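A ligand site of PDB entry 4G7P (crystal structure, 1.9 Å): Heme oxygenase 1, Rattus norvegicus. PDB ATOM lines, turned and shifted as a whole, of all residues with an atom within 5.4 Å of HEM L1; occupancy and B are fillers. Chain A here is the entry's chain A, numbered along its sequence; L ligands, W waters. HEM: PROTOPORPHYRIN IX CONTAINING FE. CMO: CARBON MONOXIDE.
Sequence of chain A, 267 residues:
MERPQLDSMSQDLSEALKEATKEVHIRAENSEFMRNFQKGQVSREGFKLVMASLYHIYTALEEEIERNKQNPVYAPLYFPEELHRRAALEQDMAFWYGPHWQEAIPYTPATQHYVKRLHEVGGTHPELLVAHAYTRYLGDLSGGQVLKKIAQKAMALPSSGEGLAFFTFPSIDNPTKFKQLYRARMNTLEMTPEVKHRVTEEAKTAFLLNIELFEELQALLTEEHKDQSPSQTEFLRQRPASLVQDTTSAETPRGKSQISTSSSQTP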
ATOM      1  N   SER A  14      -7.497 -17.945   7.773  1.00  0.00           N
ATOM      2  CA  SER A  14      -7.865 -17.758   6.365  1.00  0.00           C
ATOM      3  C   SER A  14      -8.635 -19.007   5.814  1.00  0.00           C
ATOM      4  O   SER A  14      -9.594 -18.840   5.033  1.00  0.00           O
ATOM      5  CB  SER A  14      -6.663 -17.559   5.476  1.00  0.00           C
ATOM      6  OG  SER A  14      -5.771 -18.605   5.757  1.00  0.00           O
ATOM      7  N   LEU A  17     -12.186 -19.143   7.599  1.00  0.00           N
ATOM      8  CA  LEU A  17     -13.143 -18.217   6.999  1.00  0.00           C
ATOM      9  C   LEU A  17     -13.616 -18.766   5.651  1.00  0.00           C
ATOM     10  O   LEU A  17     -14.824 -18.734   5.328  1.00  0.00           O
ATOM     11  CB  LEU A  17     -12.518 -16.828   6.794  1.00  0.00           C
ATOM     12  CG  LEU A  17     -12.498 -15.997   8.032  1.00  0.00           C
ATOM     13  CD1 LEU A  17     -11.538 -14.784   7.867  1.00  0.00           C
ATOM     14  CD2 LEU A  17     -13.914 -15.600   8.376  1.00  0.00           C
ATOM     15  N   LYS A  18     -12.694 -19.340   4.867  1.00  0.00           N
ATOM     16  CA  LYS A  18     -13.100 -19.826   3.526  1.00  0.00           C
ATOM     17  C   LYS A  18     -14.138 -20.962   3.726  1.00  0.00           C
ATOM     18  O   LYS A  18     -15.187 -21.011   3.044  1.00  0.00           O
ATOM     19  CB  LYS A  18     -11.847 -20.336   2.723  1.00  0.00           C
ATOM     20  CG  LYS A  18     -12.199 -20.588   1.231  1.00  0.00           C
ATOM     21  CD  LYS A  18     -11.023 -21.131   0.410  1.00  0.00           C
ATOM     22  CE  LYS A  18     -11.223 -20.726  -1.060  1.00  0.00           C
ATOM     23  NZ  LYS A  18     -10.620 -21.653  -2.030  1.00  0.00           N
ATOM     24  N   HIS A  25     -21.623 -18.336   0.295  1.00  0.00           N
ATOM     25  CA  HIS A  25     -21.135 -17.763  -0.978  1.00  0.00           C
ATOM     26  C   HIS A  25     -21.903 -18.255  -2.211  1.00  0.00           C
ATOM     27  O   HIS A  25     -22.335 -17.485  -3.085  1.00  0.00           O
ATOM     28  CB  HIS A  25     -19.630 -18.038  -1.141  1.00  0.00           C
ATOM     29  CG  HIS A  25     -19.075 -17.413  -2.397  1.00  0.00           C
ATOM     30  ND1 HIS A  25     -19.421 -17.837  -3.660  1.00  0.00           N
ATOM     31  CD2 HIS A  25     -18.241 -16.305  -2.566  1.00  0.00           C
ATOM     32  CE1 HIS A  25     -18.806 -17.042  -4.567  1.00  0.00           C
ATOM     33  NE2 HIS A  25     -18.113 -16.108  -3.897  1.00  0.00           N
ATOM     34  N   ALA A  28     -25.090 -16.478  -2.246  1.00  0.00           N
ATOM     35  CA  ALA A  28     -24.912 -15.085  -2.714  1.00  0.00           C
ATOM     36  C   ALA A  28     -24.811 -14.996  -4.250  1.00  0.00           C
ATOM     37  O   ALA A  28     -25.493 -14.179  -4.846  1.00  0.00           O
ATOM     38  CB  ALA A  28     -23.731 -14.350  -2.031  1.00  0.00           C
ATOM     39  N   GLU A  29     -24.045 -15.880  -4.842  1.00  0.00           N
ATOM     40  CA  GLU A  29     -23.944 -15.942  -6.310  1.00  0.00           C
ATOM     41  C   GLU A  29     -25.275 -16.182  -7.021  1.00  0.00           C
ATOM     42  O   GLU A  29     -25.468 -15.730  -8.158  1.00  0.00           O
ATOM     43  CB  GLU A  29     -23.103 -17.094  -6.728  1.00  0.00           C
ATOM     44  CG  GLU A  29     -21.681 -17.007  -6.393  1.00  0.00           C
ATOM     45  CD  GLU A  29     -21.004 -18.347  -6.688  1.00  0.00           C
ATOM     46  OE1 GLU A  29     -20.711 -18.584  -7.879  1.00  0.00           O
ATOM     47  OE2 GLU A  29     -20.770 -19.136  -5.732  1.00  0.00           O
ATOM     48  N   MET A  34     -27.555 -11.269  -8.768  1.00  0.00           N
ATOM     49  CA  MET A  34     -26.200 -11.708  -9.199  1.00  0.00           C
ATOM     50  C   MET A  34     -26.291 -12.732 -10.336  1.00  0.00           C
ATOM     51  O   MET A  34     -25.491 -12.720 -11.255  1.00  0.00           O
ATOM     52  CB  MET A  34     -25.398 -12.305  -8.057  1.00  0.00           C
ATOM     53  CG  MET A  34     -24.950 -11.324  -7.058  1.00  0.00           C
ATOM     54  SD  MET A  34     -23.666 -10.282  -7.808  1.00  0.00           S
ATOM     55  CE  MET A  34     -24.524  -8.855  -7.971  1.00  0.00           C
ATOM     56  N   ARG A  35     -27.358 -13.549 -10.286  1.00  0.00           N
ATOM     57  CA  ARG A  35     -27.640 -14.482 -11.359  1.00  0.00           C
ATOM     58  C   ARG A  35     -27.819 -13.707 -12.682  1.00  0.00           C
ATOM     59  O   ARG A  35     -27.170 -13.991 -13.679  1.00  0.00           O
ATOM     60  CB  ARG A  35     -28.925 -15.270 -11.038  1.00  0.00           C
ATOM     61  CG  ARG A  35     -28.882 -16.726 -11.384  1.00  0.00           C
ATOM     62  CD  ARG A  35     -30.043 -17.482 -10.679  1.00  0.00           C
ATOM     63  NE  ARG A  35     -31.367 -16.846 -10.886  1.00  0.00           N
ATOM     64  CZ  ARG A  35     -32.356 -16.846  -9.994  1.00  0.00           C
ATOM     65  NH1 ARG A  35     -32.223 -17.431  -8.794  1.00  0.00           N
ATOM     66  NH2 ARG A  35     -33.479 -16.250 -10.283  1.00  0.00           N
ATOM     67  N   GLN A  38     -24.461 -12.104 -13.712  1.00  0.00           N
ATOM     68  CA  GLN A  38     -23.503 -13.050 -14.277  1.00  0.00           C
ATOM     69  C   GLN A  38     -23.838 -13.482 -15.660  1.00  0.00           C
ATOM     70  O   GLN A  38     -22.940 -13.827 -16.394  1.00  0.00           O
ATOM     71  CB  GLN A  38     -23.483 -14.317 -13.508  1.00  0.00           C
ATOM     72  CG  GLN A  38     -22.675 -14.314 -12.277  1.00  0.00           C
ATOM     73  CD  GLN A  38     -22.816 -15.647 -11.575  1.00  0.00           C
ATOM     74  OE1 GLN A  38     -23.766 -15.864 -10.793  1.00  0.00           O
ATOM     75  NE2 GLN A  38     -21.872 -16.536 -11.819  1.00  0.00           N
ATOM     76  N   TYR A 134     -12.443  -9.162   5.082  1.00  0.00           N
ATOM     77  CA  TYR A 134     -12.320 -10.441   4.344  1.00  0.00           C
ATOM     78  C   TYR A 134     -13.465 -10.571   3.321  1.00  0.00           C
ATOM     79  O   TYR A 134     -13.207 -10.809   2.076  1.00  0.00           O
ATOM     80  CB  TYR A 134     -12.313 -11.661   5.333  1.00  0.00           C
ATOM     81  CG  TYR A 134     -12.599 -12.978   4.687  1.00  0.00           C
ATOM     82  CD1 TYR A 134     -11.582 -13.680   4.020  1.00  0.00           C
ATOM     83  CD2 TYR A 134     -13.903 -13.514   4.678  1.00  0.00           C
ATOM     84  CE1 TYR A 134     -11.812 -14.905   3.370  1.00  0.00           C
ATOM     85  CE2 TYR A 134     -14.141 -14.669   3.978  1.00  0.00           C
ATOM     86  CZ  TYR A 134     -13.078 -15.409   3.375  1.00  0.00           C
ATOM     87  OH  TYR A 134     -13.380 -16.607   2.728  1.00  0.00           O
ATOM     88  N   THR A 135     -14.713 -10.418   3.808  1.00  0.00           N
ATOM     89  CA  THR A 135     -15.891 -10.710   2.991  1.00  0.00           C
ATOM     90  C   THR A 135     -15.902  -9.769   1.736  1.00  0.00           C
ATOM     91  O   THR A 135     -16.223 -10.223   0.656  1.00  0.00           O
ATOM     92  CB  THR A 135     -17.188 -10.582   3.795  1.00  0.00           C
ATOM     93  OG1 THR A 135     -17.221 -11.624   4.813  1.00  0.00           O
ATOM     94  CG2 THR A 135     -18.448 -10.637   2.892  1.00  0.00           C
ATOM     95  N   ARG A 136     -15.556  -8.504   1.886  1.00  0.00           N
ATOM     96  CA  ARG A 136     -15.580  -7.574   0.770  1.00  0.00           C
ATOM     97  C   ARG A 136     -14.282  -7.662  -0.053  1.00  0.00           C
ATOM     98  O   ARG A 136     -14.326  -8.004  -1.247  1.00  0.00           O
ATOM     99  CB  ARG A 136     -15.858  -6.129   1.265  1.00  0.00           C
ATOM    100  CG  ARG A 136     -17.351  -5.765   1.592  1.00  0.00           C
ATOM    101  CD  ARG A 136     -18.419  -6.311   0.581  1.00  0.00           C
ATOM    102  NE  ARG A 136     -18.000  -6.051  -0.783  1.00  0.00           N
ATOM    103  CZ  ARG A 136     -18.665  -6.370  -1.904  1.00  0.00           C
ATOM    104  NH1 ARG A 136     -19.833  -6.900  -1.860  1.00  0.00           N
ATOM    105  NH2 ARG A 136     -18.140  -6.116  -3.107  1.00  0.00           N
ATOM    106  N   LEU A 138     -11.489  -9.685  -0.219  1.00  0.00           N
ATOM    107  CA  LEU A 138     -11.036 -10.911  -0.855  1.00  0.00           C
ATOM    108  C   LEU A 138     -11.955 -11.320  -2.012  1.00  0.00           C
ATOM    109  O   LEU A 138     -11.483 -11.921  -3.020  1.00  0.00           O
ATOM    110  CB  LEU A 138     -10.803 -12.021   0.147  1.00  0.00           C
ATOM    111  CG  LEU A 138      -9.325 -12.361   0.401  1.00  0.00           C
ATOM    112  CD1 LEU A 138      -8.463 -11.126   0.629  1.00  0.00           C
ATOM    113  CD2 LEU A 138      -9.193 -13.376   1.475  1.00  0.00           C
ATOM    114  N   GLY A 139     -13.247 -10.995  -1.888  1.00  0.00           N
ATOM    115  CA  GLY A 139     -14.187 -11.265  -2.994  1.00  0.00           C
ATOM    116  C   GLY A 139     -13.784 -10.367  -4.140  1.00  0.00           C
ATOM    117  O   GLY A 139     -13.696 -10.833  -5.303  1.00  0.00           O
ATOM    118  N   SER A 142     -10.973 -11.591  -6.232  1.00  0.00           N
ATOM    119  CA  SER A 142     -11.229 -12.938  -6.756  1.00  0.00           C
ATOM    120  C   SER A 142     -12.327 -12.775  -7.771  1.00  0.00           C
ATOM    121  O   SER A 142     -12.148 -12.307  -8.913  1.00  0.00           O
ATOM    122  CB  SER A 142     -11.744 -13.831  -5.600  1.00  0.00           C
ATOM    123  OG  SER A 142     -10.807 -13.890  -4.639  1.00  0.00           O
ATOM    124  N   GLY A 143     -13.531 -13.080  -7.335  1.00  0.00           N
ATOM    125  CA  GLY A 143     -14.657 -13.080  -8.194  1.00  0.00           C
ATOM    126  C   GLY A 143     -15.063 -11.711  -8.747  1.00  0.00           C
ATOM    127  O   GLY A 143     -15.703 -11.599  -9.790  1.00  0.00           O
ATOM    128  N   VAL A 146     -13.959 -11.222 -12.354  1.00  0.00           N
ATOM    129  CA  VAL A 146     -14.879 -11.853 -13.302  1.00  0.00           C
ATOM    130  C   VAL A 146     -16.081 -10.951 -13.534  1.00  0.00           C
ATOM    131  O   VAL A 146     -16.456 -10.696 -14.671  1.00  0.00           O
ATOM    132  CB  VAL A 146     -15.363 -13.229 -12.793  1.00  0.00           C
ATOM    133  CG1 VAL A 146     -16.459 -13.788 -13.706  1.00  0.00           C
ATOM    134  CG2 VAL A 146     -14.143 -14.160 -12.630  1.00  0.00           C
ATOM    135  N   LEU A 147     -16.666 -10.424 -12.467  1.00  0.00           N
ATOM    136  CA  LEU A 147     -17.778  -9.499 -12.589  1.00  0.00           C
ATOM    137  C   LEU A 147     -17.457  -8.208 -13.366  1.00  0.00           C
ATOM    138  O   LEU A 147     -18.248  -7.714 -14.147  1.00  0.00           O
ATOM    139  CB  LEU A 147     -18.325  -9.114 -11.219  1.00  0.00           C
ATOM    140  CG  LEU A 147     -18.884 -10.316 -10.423  1.00  0.00           C
ATOM    141  CD1 LEU A 147     -19.118  -9.838  -9.003  1.00  0.00           C
ATOM    142  CD2 LEU A 147     -20.173 -10.855 -11.114  1.00  0.00           C
ATOM    143  N   LYS A 179      -3.596 -11.672  -2.548  1.00  0.00           N
ATOM    144  CA  LYS A 179      -4.526 -12.449  -1.731  1.00  0.00           C
ATOM    145  C   LYS A 179      -3.751 -13.395  -0.897  1.00  0.00           C
ATOM    146  O   LYS A 179      -4.103 -13.570   0.243  1.00  0.00           O
ATOM    147  CB  LYS A 179      -5.486 -13.333  -2.566  1.00  0.00           C
ATOM    148  CG  LYS A 179      -6.816 -12.795  -2.985  1.00  0.00           C
ATOM    149  CD  LYS A 179      -7.756 -13.941  -3.490  1.00  0.00           C
ATOM    150  CE  LYS A 179      -7.201 -14.758  -4.644  1.00  0.00           C
ATOM    151  NZ  LYS A 179      -8.097 -15.914  -4.974  1.00  0.00           N
ATOM    152  N   ARG A 183      -3.990 -13.332   3.210  1.00  0.00           N
ATOM    153  CA  ARG A 183      -4.318 -14.494   3.998  1.00  0.00           C
ATOM    154  C   ARG A 183      -3.206 -14.786   5.012  1.00  0.00           C
ATOM    155  O   ARG A 183      -3.482 -15.098   6.158  1.00  0.00           O
ATOM    156  CB  ARG A 183      -4.496 -15.714   3.111  1.00  0.00           C
ATOM    157  CG  ARG A 183      -5.675 -15.605   2.138  1.00  0.00           C
ATOM    158  CD  ARG A 183      -5.810 -17.007   1.525  1.00  0.00           C
ATOM    159  NE  ARG A 183      -6.936 -17.096   0.604  1.00  0.00           N
ATOM    160  CZ  ARG A 183      -6.816 -17.270  -0.702  1.00  0.00           C
ATOM    161  NH1 ARG A 183      -5.620 -17.404  -1.275  1.00  0.00           N
ATOM    162  NH2 ARG A 183      -7.907 -17.409  -1.439  1.00  0.00           N
ATOM    163  N   ALA A 206     -21.857 -10.872   7.371  1.00  0.00           N
ATOM    164  CA  ALA A 206     -21.441  -9.954   6.287  1.00  0.00           C
ATOM    165  C   ALA A 206     -22.015 -10.436   4.911  1.00  0.00           C
ATOM    166  O   ALA A 206     -22.547  -9.661   4.138  1.00  0.00           O
ATOM    167  CB  ALA A 206     -19.929  -9.970   6.258  1.00  0.00           C
ATOM    168  N   PHE A 207     -21.896 -11.740   4.654  1.00  0.00           N
ATOM    169  CA  PHE A 207     -22.442 -12.363   3.470  1.00  0.00           C
ATOM    170  C   PHE A 207     -23.954 -12.166   3.431  1.00  0.00           C
ATOM    171  O   PHE A 207     -24.456 -11.798   2.404  1.00  0.00           O
ATOM    172  CB  PHE A 207     -22.109 -13.839   3.361  1.00  0.00           C
ATOM    173  CG  PHE A 207     -20.860 -14.130   2.611  1.00  0.00           C
ATOM    174  CD1 PHE A 207     -19.640 -14.214   3.247  1.00  0.00           C
ATOM    175  CD2 PHE A 207     -20.902 -14.310   1.218  1.00  0.00           C
ATOM    176  CE1 PHE A 207     -18.488 -14.480   2.558  1.00  0.00           C
ATOM    177  CE2 PHE A 207     -19.742 -14.555   0.541  1.00  0.00           C
ATOM    178  CZ  PHE A 207     -18.524 -14.619   1.186  1.00  0.00           C
ATOM    179  N   ASN A 210     -24.942  -8.666   2.449  1.00  0.00           N
ATOM    180  CA  ASN A 210     -24.822  -8.538   1.016  1.00  0.00           C
ATOM    181  C   ASN A 210     -26.038  -9.173   0.220  1.00  0.00           C
ATOM    182  O   ASN A 210     -26.601  -8.538  -0.698  1.00  0.00           O
ATOM    183  CB  ASN A 210     -23.525  -9.140   0.537  1.00  0.00           C
ATOM    184  CG  ASN A 210     -22.329  -8.200   0.762  1.00  0.00           C
ATOM    185  OD1 ASN A 210     -22.017  -7.279  -0.071  1.00  0.00           O
ATOM    186  ND2 ASN A 210     -21.611  -8.460   1.901  1.00  0.00           N
ATOM    187  N   PHE A 214     -28.771  -7.335  -2.192  1.00  0.00           N
ATOM    188  CA  PHE A 214     -29.095  -7.837  -3.545  1.00  0.00           C
ATOM    189  C   PHE A 214     -30.578  -8.149  -3.678  1.00  0.00           C
ATOM    190  O   PHE A 214     -31.220  -7.777  -4.708  1.00  0.00           O
ATOM    191  CB  PHE A 214     -28.280  -9.070  -3.976  1.00  0.00           C
ATOM    192  CG  PHE A 214     -26.802  -8.857  -3.966  1.00  0.00           C
ATOM    193  CD1 PHE A 214     -26.247  -7.611  -4.209  1.00  0.00           C
ATOM    194  CD2 PHE A 214     -25.960  -9.915  -3.679  1.00  0.00           C
ATOM    195  CE1 PHE A 214     -24.853  -7.392  -4.166  1.00  0.00           C
ATOM    196  CE2 PHE A 214     -24.557  -9.696  -3.625  1.00  0.00           C
ATOM    197  CZ  PHE A 214     -24.029  -8.450  -3.911  1.00  0.00           C
HETATM  198  CHA HEM L   1     -13.933 -15.910  -3.964  1.00  0.00           C
HETATM  199  CHB HEM L   1     -17.193 -15.622  -7.893  1.00  0.00           C
HETATM  200  CHC HEM L   1     -20.248 -13.032  -5.313  1.00  0.00           C
HETATM  201  CHD HEM L   1     -17.057 -12.951  -1.567  1.00  0.00           C
HETATM  202  C1A HEM L   1     -14.620 -16.068  -5.246  1.00  0.00           C
HETATM  203  C2A HEM L   1     -14.009 -16.742  -6.413  1.00  0.00           C
HETATM  204  C3A HEM L   1     -14.912 -16.670  -7.531  1.00  0.00           C
HETATM  205  C4A HEM L   1     -16.084 -15.904  -6.958  1.00  0.00           C
HETATM  206  CMA HEM L   1     -14.704 -17.259  -8.946  1.00  0.00           C
HETATM  207  CAA HEM L   1     -12.694 -17.398  -6.318  1.00  0.00           C
HETATM  208  CBA HEM L   1     -12.946 -18.775  -5.707  1.00  0.00           C
HETATM  209  CGA HEM L   1     -11.631 -19.523  -5.462  1.00  0.00           C
HETATM  210  O1A HEM L   1     -10.587 -18.867  -5.627  1.00  0.00           O
HETATM  211  O2A HEM L   1     -11.648 -20.718  -5.078  1.00  0.00           O
HETATM  212  C1B HEM L   1     -18.330 -14.852  -7.587  1.00  0.00           C
HETATM  213  C2B HEM L   1     -19.445 -14.661  -8.533  1.00  0.00           C
HETATM  214  C3B HEM L   1     -20.301 -13.894  -7.680  1.00  0.00           C
HETATM  215  C4B HEM L   1     -19.594 -13.725  -6.406  1.00  0.00           C
HETATM  216  CMB HEM L   1     -19.624 -15.156  -9.933  1.00  0.00           C
HETATM  217  CAB HEM L   1     -21.663 -13.389  -7.962  1.00  0.00           C
HETATM  218  CBB HEM L   1     -22.266 -13.845  -9.039  1.00  0.00           C
HETATM  219  C1C HEM L   1     -19.668 -12.749  -4.030  1.00  0.00           C
HETATM  220  C2C HEM L   1     -20.388 -11.938  -3.032  1.00  0.00           C
HETATM  221  C3C HEM L   1     -19.383 -11.945  -1.963  1.00  0.00           C
HETATM  222  C4C HEM L   1     -18.189 -12.661  -2.373  1.00  0.00           C
HETATM  223  CMC HEM L   1     -21.754 -11.363  -3.193  1.00  0.00           C
HETATM  224  CAC HEM L   1     -19.381 -11.265  -0.689  1.00  0.00           C
HETATM  225  CBC HEM L   1     -20.205 -10.321  -0.463  1.00  0.00           C
HETATM  226  C1D HEM L   1     -15.924 -13.751  -1.923  1.00  0.00           C
HETATM  227  C2D HEM L   1     -14.876 -13.935  -0.913  1.00  0.00           C
HETATM  228  C3D HEM L   1     -13.969 -14.781  -1.633  1.00  0.00           C
HETATM  229  C4D HEM L   1     -14.558 -15.005  -2.957  1.00  0.00           C
HETATM  230  CMD HEM L   1     -14.657 -13.438   0.490  1.00  0.00           C
HETATM  231  CAD HEM L   1     -12.676 -15.322  -1.137  1.00  0.00           C
HETATM  232  CBD HEM L   1     -12.849 -16.744  -0.709  1.00  0.00           C
HETATM  233  CGD HEM L   1     -11.538 -17.145  -0.039  1.00  0.00           C
HETATM  234  O1D HEM L   1     -10.574 -17.358  -0.785  1.00  0.00           O
HETATM  235  O2D HEM L   1     -11.425 -17.342   1.195  1.00  0.00           O
HETATM  236  NA  HEM L   1     -15.959 -15.611  -5.537  1.00  0.00           N
HETATM  237  NB  HEM L   1     -18.430 -14.358  -6.315  1.00  0.00           N
HETATM  238  NC  HEM L   1     -18.441 -13.292  -3.580  1.00  0.00           N
HETATM  239  ND  HEM L   1     -15.783 -14.424  -3.124  1.00  0.00           N
HETATM  240 FE   HEM L   1     -17.120 -14.247  -4.694  1.00  0.00          FE
HETATM  241  C   CMO L   2     -16.342 -12.605  -5.564  1.00  0.00           C
HETATM  242  O   CMO L   2     -16.315 -11.422  -5.626  1.00  0.00           O
HETATM  243  O   HOH W   1     -18.092  -9.695  -4.485  1.00  0.00           O
HETATM  244  O   HOH W   2     -15.884 -18.905  -4.025  1.00  0.00           O
HETATM  245  O   HOH W   3      -9.174 -17.700   2.637  1.00  0.00           O
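Residues that only touch HEM L1: Ala 28 (3.8 Å), Glu 29 (3.6 Å), Met 34 (3.6 Å), Gln 38 (3.1 Å), Thr 135 (3.6 Å), Arg 136 (3.7 Å), Gly 139 (3.2 Å), Ser 142 (3.4 Å), Gly 143 (3.4 Å), Phe 207 (3.5 Å), Asn 210 (3.2 Å) and Phe 214 (3.3 Å). Hydrophobic or aromatic side chains that line HEM L1: His 25, Ala 28, Met 34, Tyr 134, Phe 207 and Phe 214. Along chain A the residues within 4 Å of HEM L1 span positions 18 to 214.
O of Glu 29 lies close to OE1 of Gln 38 (3.1 Å). The side-chain carboxylate (OE2) of Glu 29 lies within hydrogen-bond range of a ring nitrogen (ND1) of His 25, 2.8 Å away. The backbone carbonyl oxygen (O) of Leu 138 lies within hydrogen-bond range of the side-chain hydroxyl (OG) of Ser 142 (2.6 Å). OG of Ser 142 sits close to NZ of Lys 179, at 3.4 Å. The backbone carbonyl oxygen of Ala 206 lies within hydrogen-bond range of the side-chain amide nitrogen of Asn 210 (2.7 Å). The guanidinium group of Arg 136 sits at hydrogen-bond distance from the side-chain amide oxygen of Asn 210, at 2.8 Å.
An oxygen (O2A) of HEM L1 is in salt-bridge range of the side-chain amino group of Lys 18, 3.3 Å away. NE2 of His 25 binds FE of HEM L1 (2.3 Å). O1D of HEM L1 lies within salt-bridge range of NH2 of Arg 183, 2.7 Å away. An oxygen (O2D) of HEM L1 lies within hydrogen-bond range of the side-chain hydroxyl of Tyr 134 (2.6 Å). O1A of HEM L1 lies within salt-bridge range of NZ of Lys 179 (3.9 Å). The backbone carbonyl oxygen of Gly 139 lies close to an oxygen (O) of CMO L2 (2.7 Å).
Water W3 lies within hydrogen-bond range of O of Ser 14 (2.7 Å), O2D of HEM L1 (2.7 Å) and NE of Arg 183 (3.1 Å).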
